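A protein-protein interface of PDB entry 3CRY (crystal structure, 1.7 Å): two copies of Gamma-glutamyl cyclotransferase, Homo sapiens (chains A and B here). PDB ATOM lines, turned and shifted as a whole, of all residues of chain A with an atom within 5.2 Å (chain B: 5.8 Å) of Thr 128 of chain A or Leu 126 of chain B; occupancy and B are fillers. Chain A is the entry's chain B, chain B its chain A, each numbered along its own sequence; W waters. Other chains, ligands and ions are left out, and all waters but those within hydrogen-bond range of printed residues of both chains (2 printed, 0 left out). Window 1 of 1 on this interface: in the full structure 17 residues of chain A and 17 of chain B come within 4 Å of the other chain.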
ATOM      1  N   GLN A  73      30.460 -17.381  10.191  1.00  0.00           N
ATOM      2  CA  GLN A  73      31.789 -17.106  10.748  1.00  0.00           C
ATOM      3  C   GLN A  73      32.472 -18.382  11.197  1.00  0.00           C
ATOM      4  O   GLN A  73      31.876 -19.203  11.905  1.00  0.00           O
ATOM      5  CB  GLN A  73      31.677 -16.107  11.889  1.00  0.00           C
ATOM      6  CG  GLN A  73      31.194 -14.735  11.425  1.00  0.00           C
ATOM      7  CD  GLN A  73      30.615 -13.908  12.561  1.00  0.00           C
ATOM      8  OE1 GLN A  73      29.647 -14.315  13.211  1.00  0.00           O
ATOM      9  NE2 GLN A  73      31.185 -12.724  12.779  1.00  0.00           N
ATOM     10  N   MET A 104      14.528 -14.660   4.176  1.00  0.00           N
ATOM     11  CA  MET A 104      15.464 -15.529   3.465  1.00  0.00           C
ATOM     12  C   MET A 104      16.902 -15.173   3.818  1.00  0.00           C
ATOM     13  O   MET A 104      17.720 -16.056   4.129  1.00  0.00           O
ATOM     14  CB  MET A 104      15.265 -15.433   1.955  1.00  0.00           C
ATOM     15  CG  MET A 104      15.939 -16.544   1.173  1.00  0.00           C
ATOM     16  SD  MET A 104      15.609 -16.464  -0.603  1.00  0.00           S
ATOM     17  CE  MET A 104      13.834 -16.285  -0.607  1.00  0.00           C
ATOM     18  N   VAL A 106      19.465 -11.901   5.821  1.00  0.00           N
ATOM     19  CA  VAL A 106      19.580 -10.652   6.578  1.00  0.00           C
ATOM     20  C   VAL A 106      20.685  -9.801   5.951  1.00  0.00           C
ATOM     21  O   VAL A 106      21.668 -10.348   5.422  1.00  0.00           O
ATOM     22  CB  VAL A 106      19.858 -10.952   8.091  1.00  0.00           C
ATOM     23  CG1 VAL A 106      21.298 -11.495   8.303  1.00  0.00           C
ATOM     24  CG2 VAL A 106      19.599  -9.678   8.943  1.00  0.00           C
ATOM     25  N   LEU A 126      23.413 -12.749   4.434  1.00  0.00           N
ATOM     26  CA  LEU A 126      23.569 -14.163   4.782  1.00  0.00           C
ATOM     27  C   LEU A 126      22.286 -14.739   5.393  1.00  0.00           C
ATOM     28  O   LEU A 126      21.407 -13.968   5.803  1.00  0.00           O
ATOM     29  CB  LEU A 126      24.801 -14.405   5.669  1.00  0.00           C
ATOM     30  CG  LEU A 126      24.841 -13.743   7.068  1.00  0.00           C
ATOM     31  CD1 LEU A 126      23.816 -14.313   8.046  1.00  0.00           C
ATOM     32  CD2 LEU A 126      26.241 -13.867   7.648  1.00  0.00           C
ATOM     33  N   MET A 127      22.170 -16.074   5.393  1.00  0.00           N
ATOM     34  CA  MET A 127      20.994 -16.728   5.976  1.00  0.00           C
ATOM     35  C   MET A 127      21.179 -16.967   7.482  1.00  0.00           C
ATOM     36  O   MET A 127      22.265 -17.350   7.940  1.00  0.00           O
ATOM     37  CB  MET A 127      20.672 -18.034   5.237  1.00  0.00           C
ATOM     38  CG  MET A 127      20.315 -17.798   3.774  1.00  0.00           C
ATOM     39  SD  MET A 127      19.377 -19.109   2.978  1.00  0.00           S
ATOM     40  CE  MET A 127      20.654 -20.343   2.920  1.00  0.00           C
ATOM     41  N   THR A 128      20.106 -16.742   8.238  1.00  0.00           N
ATOM     42  CA  THR A 128      20.173 -16.950   9.696  1.00  0.00           C
ATOM     43  C   THR A 128      19.414 -18.182  10.195  1.00  0.00           C
ATOM     44  O   THR A 128      19.549 -18.558  11.371  1.00  0.00           O
ATOM     45  CB  THR A 128      19.655 -15.723  10.481  1.00  0.00           C
ATOM     46  OG1 THR A 128      18.242 -15.572  10.285  1.00  0.00           O
ATOM     47  CG2 THR A 128      20.366 -14.420  10.048  1.00  0.00           C
ATOM     48  N   ASN A 129      18.583 -18.760   9.331  1.00  0.00           N
ATOM     49  CA  ASN A 129      17.786 -19.922   9.694  1.00  0.00           C
ATOM     50  C   ASN A 129      17.625 -20.780   8.455  1.00  0.00           C
ATOM     51  O   ASN A 129      16.804 -20.475   7.575  1.00  0.00           O
ATOM     52  CB  ASN A 129      16.409 -19.506  10.235  1.00  0.00           C
ATOM     53  CG  ASN A 129      15.677 -20.665  10.893  1.00  0.00           C
ATOM     54  OD1 ASN A 129      16.066 -21.831  10.729  1.00  0.00           O
ATOM     55  ND2 ASN A 129      14.612 -20.359  11.637  1.00  0.00           N
ATOM     56  N   TYR A 130      18.449 -21.818   8.374  1.00  0.00           N
ATOM     57  CA  TYR A 130      18.482 -22.651   7.168  1.00  0.00           C
ATOM     58  C   TYR A 130      18.929 -24.071   7.440  1.00  0.00           C
ATOM     59  O   TYR A 130      19.546 -24.357   8.475  1.00  0.00           O
ATOM     60  CB  TYR A 130      19.389 -22.013   6.081  1.00  0.00           C
ATOM     61  CG  TYR A 130      20.899 -22.171   6.307  1.00  0.00           C
ATOM     62  CD1 TYR A 130      21.608 -21.277   7.137  1.00  0.00           C
ATOM     63  CD2 TYR A 130      21.611 -23.189   5.669  1.00  0.00           C
ATOM     64  CE1 TYR A 130      22.991 -21.424   7.342  1.00  0.00           C
ATOM     65  CE2 TYR A 130      22.981 -23.351   5.876  1.00  0.00           C
ATOM     66  CZ  TYR A 130      23.665 -22.458   6.706  1.00  0.00           C
ATOM     67  OH  TYR A 130      25.024 -22.611   6.889  1.00  0.00           O
ATOM     68  N   TYR B  22      19.007  -5.724  22.076  1.00  0.00           N
ATOM     69  CA  TYR B  22      18.019  -6.678  22.576  1.00  0.00           C
ATOM     70  C   TYR B  22      18.490  -7.553  23.764  1.00  0.00           C
ATOM     71  O   TYR B  22      17.721  -8.391  24.267  1.00  0.00           O
ATOM     72  CB  TYR B  22      17.545  -7.567  21.408  1.00  0.00           C
ATOM     73  CG  TYR B  22      18.665  -8.296  20.707  1.00  0.00           C
ATOM     74  CD1 TYR B  22      19.188  -9.502  21.239  1.00  0.00           C
ATOM     75  CD2 TYR B  22      19.220  -7.790  19.527  1.00  0.00           C
ATOM     76  CE1 TYR B  22      20.238 -10.163  20.622  1.00  0.00           C
ATOM     77  CE2 TYR B  22      20.280  -8.472  18.871  1.00  0.00           C
ATOM     78  CZ  TYR B  22      20.776  -9.644  19.435  1.00  0.00           C
ATOM     79  OH  TYR B  22      21.804 -10.317  18.821  1.00  0.00           O
ATOM     80  N   PHE B  49      11.715 -12.119  13.851  1.00  0.00           N
ATOM     81  CA  PHE B  49      12.934 -12.660  14.459  1.00  0.00           C
ATOM     82  C   PHE B  49      12.570 -13.241  15.819  1.00  0.00           C
ATOM     83  O   PHE B  49      11.546 -12.835  16.418  1.00  0.00           O
ATOM     84  CB  PHE B  49      13.972 -11.556  14.692  1.00  0.00           C
ATOM     85  CG  PHE B  49      14.772 -11.165  13.464  1.00  0.00           C
ATOM     86  CD1 PHE B  49      14.197 -10.392  12.455  1.00  0.00           C
ATOM     87  CD2 PHE B  49      16.131 -11.521  13.354  1.00  0.00           C
ATOM     88  CE1 PHE B  49      14.945 -10.001  11.340  1.00  0.00           C
ATOM     89  CE2 PHE B  49      16.870 -11.133  12.239  1.00  0.00           C
ATOM     90  CZ  PHE B  49      16.284 -10.369  11.248  1.00  0.00           C
ATOM     91  N   THR B  70      21.235 -13.723  21.216  1.00  0.00           N
ATOM     92  CA  THR B  70      21.285 -13.617  19.743  1.00  0.00           C
ATOM     93  C   THR B  70      19.865 -13.628  19.177  1.00  0.00           C
ATOM     94  O   THR B  70      18.895 -13.860  19.912  1.00  0.00           O
ATOM     95  CB  THR B  70      22.178 -14.724  19.119  1.00  0.00           C
ATOM     96  OG1 THR B  70      22.346 -14.481  17.704  1.00  0.00           O
ATOM     97  CG2 THR B  70      21.534 -16.131  19.320  1.00  0.00           C
ATOM     98  N   ILE B  71      19.733 -13.340  17.889  1.00  0.00           N
ATOM     99  CA  ILE B  71      18.412 -13.358  17.219  1.00  0.00           C
ATOM    100  C   ILE B  71      18.570 -14.065  15.886  1.00  0.00           C
ATOM    101  O   ILE B  71      19.675 -14.095  15.303  1.00  0.00           O
ATOM    102  CB  ILE B  71      17.815 -11.940  17.010  1.00  0.00           C
ATOM    103  CG1 ILE B  71      18.786 -11.033  16.217  1.00  0.00           C
ATOM    104  CG2 ILE B  71      17.438 -11.301  18.384  1.00  0.00           C
ATOM    105  CD1 ILE B  71      18.252  -9.617  15.875  1.00  0.00           C
ATOM    106  N   PHE B  72      17.483 -14.674  15.424  1.00  0.00           N
ATOM    107  CA  PHE B  72      17.508 -15.311  14.104  1.00  0.00           C
ATOM    108  C   PHE B  72      16.152 -15.177  13.419  1.00  0.00           C
ATOM    109  O   PHE B  72      15.136 -14.959  14.086  1.00  0.00           O
ATOM    110  CB  PHE B  72      18.010 -16.761  14.184  1.00  0.00           C
ATOM    111  CG  PHE B  72      17.110 -17.705  14.963  1.00  0.00           C
ATOM    112  CD1 PHE B  72      15.948 -18.234  14.382  1.00  0.00           C
ATOM    113  CD2 PHE B  72      17.457 -18.106  16.258  1.00  0.00           C
ATOM    114  CE1 PHE B  72      15.135 -19.130  15.098  1.00  0.00           C
ATOM    115  CE2 PHE B  72      16.655 -19.003  16.979  1.00  0.00           C
ATOM    116  CZ  PHE B  72      15.500 -19.513  16.406  1.00  0.00           C
ATOM    117  N   GLN B  73      16.143 -15.243  12.090  1.00  0.00           N
ATOM    118  CA  GLN B  73      14.885 -15.047  11.349  1.00  0.00           C
ATOM    119  C   GLN B  73      13.882 -16.180  11.581  1.00  0.00           C
ATOM    120  O   GLN B  73      14.221 -17.374  11.486  1.00  0.00           O
ATOM    121  CB  GLN B  73      15.196 -14.821   9.863  1.00  0.00           C
ATOM    122  CG  GLN B  73      15.838 -13.457   9.643  1.00  0.00           C
ATOM    123  CD  GLN B  73      16.529 -13.349   8.325  1.00  0.00           C
ATOM    124  OE1 GLN B  73      17.427 -14.149   8.018  1.00  0.00           O
ATOM    125  NE2 GLN B  73      16.126 -12.348   7.529  1.00  0.00           N
ATOM    126  N   MET B 104      32.430 -13.641  16.887  1.00  0.00           N
ATOM    127  CA  MET B 104      31.384 -13.840  17.896  1.00  0.00           C
ATOM    128  C   MET B 104      29.999 -13.389  17.411  1.00  0.00           C
ATOM    129  O   MET B 104      28.995 -14.091  17.610  1.00  0.00           O
ATOM    130  CB  MET B 104      31.767 -13.238  19.268  1.00  0.00           C
ATOM    131  CG  MET B 104      33.073 -13.861  19.845  1.00  0.00           C
ATOM    132  SD  MET B 104      33.069 -15.692  20.066  1.00  0.00           S
ATOM    133  CE  MET B 104      32.375 -15.827  21.724  1.00  0.00           C
ATOM    134  N   TYR B 105      29.966 -12.212  16.794  1.00  0.00           N
ATOM    135  CA  TYR B 105      28.767 -11.652  16.175  1.00  0.00           C
ATOM    136  C   TYR B 105      29.151 -11.075  14.821  1.00  0.00           C
ATOM    137  O   TYR B 105      30.318 -10.726  14.584  1.00  0.00           O
ATOM    138  CB  TYR B 105      28.203 -10.509  17.025  1.00  0.00           C
ATOM    139  CG  TYR B 105      27.536 -10.920  18.343  1.00  0.00           C
ATOM    140  CD1 TYR B 105      28.295 -11.100  19.497  1.00  0.00           C
ATOM    141  CD2 TYR B 105      26.165 -11.103  18.424  1.00  0.00           C
ATOM    142  CE1 TYR B 105      27.695 -11.439  20.709  1.00  0.00           C
ATOM    143  CE2 TYR B 105      25.536 -11.451  19.635  1.00  0.00           C
ATOM    144  CZ  TYR B 105      26.314 -11.624  20.767  1.00  0.00           C
ATOM    145  OH  TYR B 105      25.728 -11.959  21.951  1.00  0.00           O
ATOM    146  N   VAL B 106      28.152 -10.965  13.944  1.00  0.00           N
ATOM    147  CA  VAL B 106      28.285 -10.224  12.697  1.00  0.00           C
ATOM    148  C   VAL B 106      27.440  -8.952  12.797  1.00  0.00           C
ATOM    149  O   VAL B 106      26.410  -8.932  13.525  1.00  0.00           O
ATOM    150  CB  VAL B 106      27.881 -11.100  11.479  1.00  0.00           C
ATOM    151  CG1 VAL B 106      26.364 -11.323  11.458  1.00  0.00           C
ATOM    152  CG2 VAL B 106      28.371 -10.455  10.174  1.00  0.00           C
ATOM    153  N   VAL B 107      27.884  -7.881  12.125  1.00  0.00           N
ATOM    154  CA  VAL B 107      27.089  -6.657  12.010  1.00  0.00           C
ATOM    155  C   VAL B 107      25.928  -6.869  11.051  1.00  0.00           C
ATOM    156  O   VAL B 107      26.133  -7.372   9.941  1.00  0.00           O
ATOM    157  CB  VAL B 107      27.941  -5.450  11.481  1.00  0.00           C
ATOM    158  CG1 VAL B 107      27.059  -4.234  11.256  1.00  0.00           C
ATOM    159  CG2 VAL B 107      29.094  -5.144  12.410  1.00  0.00           C
ATOM    160  N   ILE B 108      24.725  -6.506  11.483  1.00  0.00           N
ATOM    161  CA  ILE B 108      23.534  -6.530  10.605  1.00  0.00           C
ATOM    162  C   ILE B 108      22.889  -5.146  10.477  1.00  0.00           C
ATOM    163  O   ILE B 108      23.166  -4.231  11.270  1.00  0.00           O
ATOM    164  CB  ILE B 108      22.464  -7.535  11.106  1.00  0.00           C
ATOM    165  CG1 ILE B 108      21.915  -7.144  12.493  1.00  0.00           C
ATOM    166  CG2 ILE B 108      23.010  -8.980  11.065  1.00  0.00           C
ATOM    167  CD1 ILE B 108      20.826  -8.110  12.994  1.00  0.00           C
ATOM    168  N   SER B 124      22.624  -3.511  14.178  1.00  0.00           N
ATOM    169  CA  SER B 124      22.555  -4.483  15.274  1.00  0.00           C
ATOM    170  C   SER B 124      23.593  -5.573  15.027  1.00  0.00           C
ATOM    171  O   SER B 124      24.499  -5.390  14.183  1.00  0.00           O
ATOM    172  CB  SER B 124      21.124  -5.067  15.413  1.00  0.00           C
ATOM    173  OG  SER B 124      20.933  -5.617  16.721  1.00  0.00           O
ATOM    174  N   TYR B 125      23.466  -6.688  15.757  1.00  0.00           N
ATOM    175  CA  TYR B 125      24.435  -7.796  15.772  1.00  0.00           C
ATOM    176  C   TYR B 125      23.696  -9.083  16.004  1.00  0.00           C
ATOM    177  O   TYR B 125      22.711  -9.100  16.747  1.00  0.00           O
ATOM    178  CB  TYR B 125      25.449  -7.629  16.915  1.00  0.00           C
ATOM    179  CG  TYR B 125      26.256  -6.354  16.782  1.00  0.00           C
ATOM    180  CD1 TYR B 125      27.456  -6.347  16.065  1.00  0.00           C
ATOM    181  CD2 TYR B 125      25.795  -5.153  17.336  1.00  0.00           C
ATOM    182  CE1 TYR B 125      28.198  -5.169  15.919  1.00  0.00           C
ATOM    183  CE2 TYR B 125      26.528  -3.971  17.193  1.00  0.00           C
ATOM    184  CZ  TYR B 125      27.723  -3.998  16.480  1.00  0.00           C
ATOM    185  OH  TYR B 125      28.431  -2.837  16.341  1.00  0.00           O
ATOM    186  N   LEU B 126      24.168 -10.155  15.362  1.00  0.00           N
ATOM    187  CA  LEU B 126      23.716 -11.499  15.740  1.00  0.00           C
ATOM    188  C   LEU B 126      24.804 -12.554  15.527  1.00  0.00           C
ATOM    189  O   LEU B 126      25.794 -12.302  14.818  1.00  0.00           O
ATOM    190  CB  LEU B 126      22.400 -11.845  15.024  1.00  0.00           C
ATOM    191  CG  LEU B 126      22.425 -11.842  13.477  1.00  0.00           C
ATOM    192  CD1 LEU B 126      23.201 -13.008  12.878  1.00  0.00           C
ATOM    193  CD2 LEU B 126      20.971 -11.833  12.956  1.00  0.00           C
ATOM    194  N   MET B 127      24.647 -13.720  16.163  1.00  0.00           N
ATOM    195  CA  MET B 127      25.638 -14.803  16.034  1.00  0.00           C
ATOM    196  C   MET B 127      25.353 -15.607  14.762  1.00  0.00           C
ATOM    197  O   MET B 127      24.185 -15.841  14.433  1.00  0.00           O
ATOM    198  CB  MET B 127      25.528 -15.750  17.225  1.00  0.00           C
ATOM    199  CG  MET B 127      25.832 -15.115  18.543  1.00  0.00           C
ATOM    200  SD  MET B 127      25.558 -16.347  19.869  1.00  0.00           S
ATOM    201  CE  MET B 127      25.815 -15.275  21.268  1.00  0.00           C
ATOM    202  N   THR B 128      26.402 -16.046  14.069  1.00  0.00           N
ATOM    203  CA  THR B 128      26.224 -16.890  12.882  1.00  0.00           C
ATOM    204  C   THR B 128      26.662 -18.341  13.074  1.00  0.00           C
ATOM    205  O   THR B 128      26.362 -19.196  12.221  1.00  0.00           O
ATOM    206  CB  THR B 128      26.984 -16.333  11.651  1.00  0.00           C
ATOM    207  OG1 THR B 128      28.397 -16.374  11.896  1.00  0.00           O
ATOM    208  CG2 THR B 128      26.579 -14.887  11.350  1.00  0.00           C
HETATM  209  O   HOH W   1      17.498 -16.998   6.955  1.00  0.00           O
HETATM  210  O   HOH W   2      28.938 -16.491  15.554  1.00  0.00           O
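The backbone NH (N) of Gln 73 of chain B sits at hydrogen-bond distance from the side-chain hydroxyl (OG1) of Thr 128 of chain A (2.8 Å).
O of Gln 73 of chain B is in hydrogen-bond range of ND2 of Asn 129 of chain A.
The backbone carbonyl oxygen (O) of Tyr 105 of chain B is in hydrogen-bond range of the side-chain amide nitrogen (NE2) of Gln 73 of chain A, at 2.8 Å.
OG1 of Thr 128 of chain B lies within hydrogen-bond range of OE1 of Gln 73 of chain A (2.7 Å).
The backbone carbonyl oxygen (O) of Leu 126 of chain B lies within hydrogen-bond range of the backbone NH (N) of Val 106 of chain B (2.8 Å).
N of Val 106 of chain A sits at hydrogen-bond distance from O of Leu 126 of chain A (2.8 Å).
Among the printed residues, merely in contact across the chains: Thr 128 of chain A with Phe 72 of chain B, Gln 73 of chain A with Val 106 of chain B, Asn 129 of chain A with Phe 72 of chain B, Val 106 of chain A with Gln 73 of chain B, Leu 126 of chain A with Thr 128 of chain B and Thr 128 of chain A with Leu 126 of chain B.
Thr 128 of chain A touches three residues of chain B.
Printed residues of chain B within 4 Å of Asn 129 of chain A: Phe 72 (3.7 Å) and Gln 73 (3.0 Å).
Printed residues of chain A within 4 Å of Val 106 of chain B: Gln 73 (3.7 Å).
Printed residues of chain A within 4 Å of Leu 126 of chain B: Thr 128 (3.9 Å).
Printed residues of chain A within 4 Å of Thr 128 of chain B: Gln 73 and Leu 126.
The nearest residue of chain A that does not touch Leu 126 of chain B is Gln 73 of chain A (4.6 Å).
The nearest printed residue of chain B that does not touch Gln 73 of chain A is Met 104 of chain B (4.3 Å).
Hydrophobic or aromatic side chains of chain B that line the printed part of chain A: Phe 72, Val 106 and Leu 126.
Among the printed residues, no Asp or Glu carboxylate lies within 4 Å of a Lys or Arg side-chain nitrogen of the other chain.
Gln 73 of chain A touches Val 106 of chain B, and with the chains exchanged Val 106 of chain A touches Gln 73 of chain B.
Gln 73 of chain A touches Thr 128 of chain B, and with the chains exchanged Thr 128 of chain A touches Gln 73 of chain B.
Leu 126 of chain A touches Thr 128 of chain B, and with the chains exchanged Thr 128 of chain A touches Leu 126 of chain B.
Water W1 lies within hydrogen-bond range of the backbone NH of Thr 128 of chain A, the backbone carbonyl oxygen of Met 104 of chain A, the side-chain amide oxygen of Gln 73 of chain B and the backbone NH of Asn 129 of chain A.
Water W2 lies within hydrogen-bond range of the backbone NH (N) of Thr 128 of chain B (3.0 Å), the backbone carbonyl oxygen (O) of Met 104 of chain B (3.2 Å) and the side-chain amide oxygen (OE1) of Gln 73 of chain A (3.3 Å).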
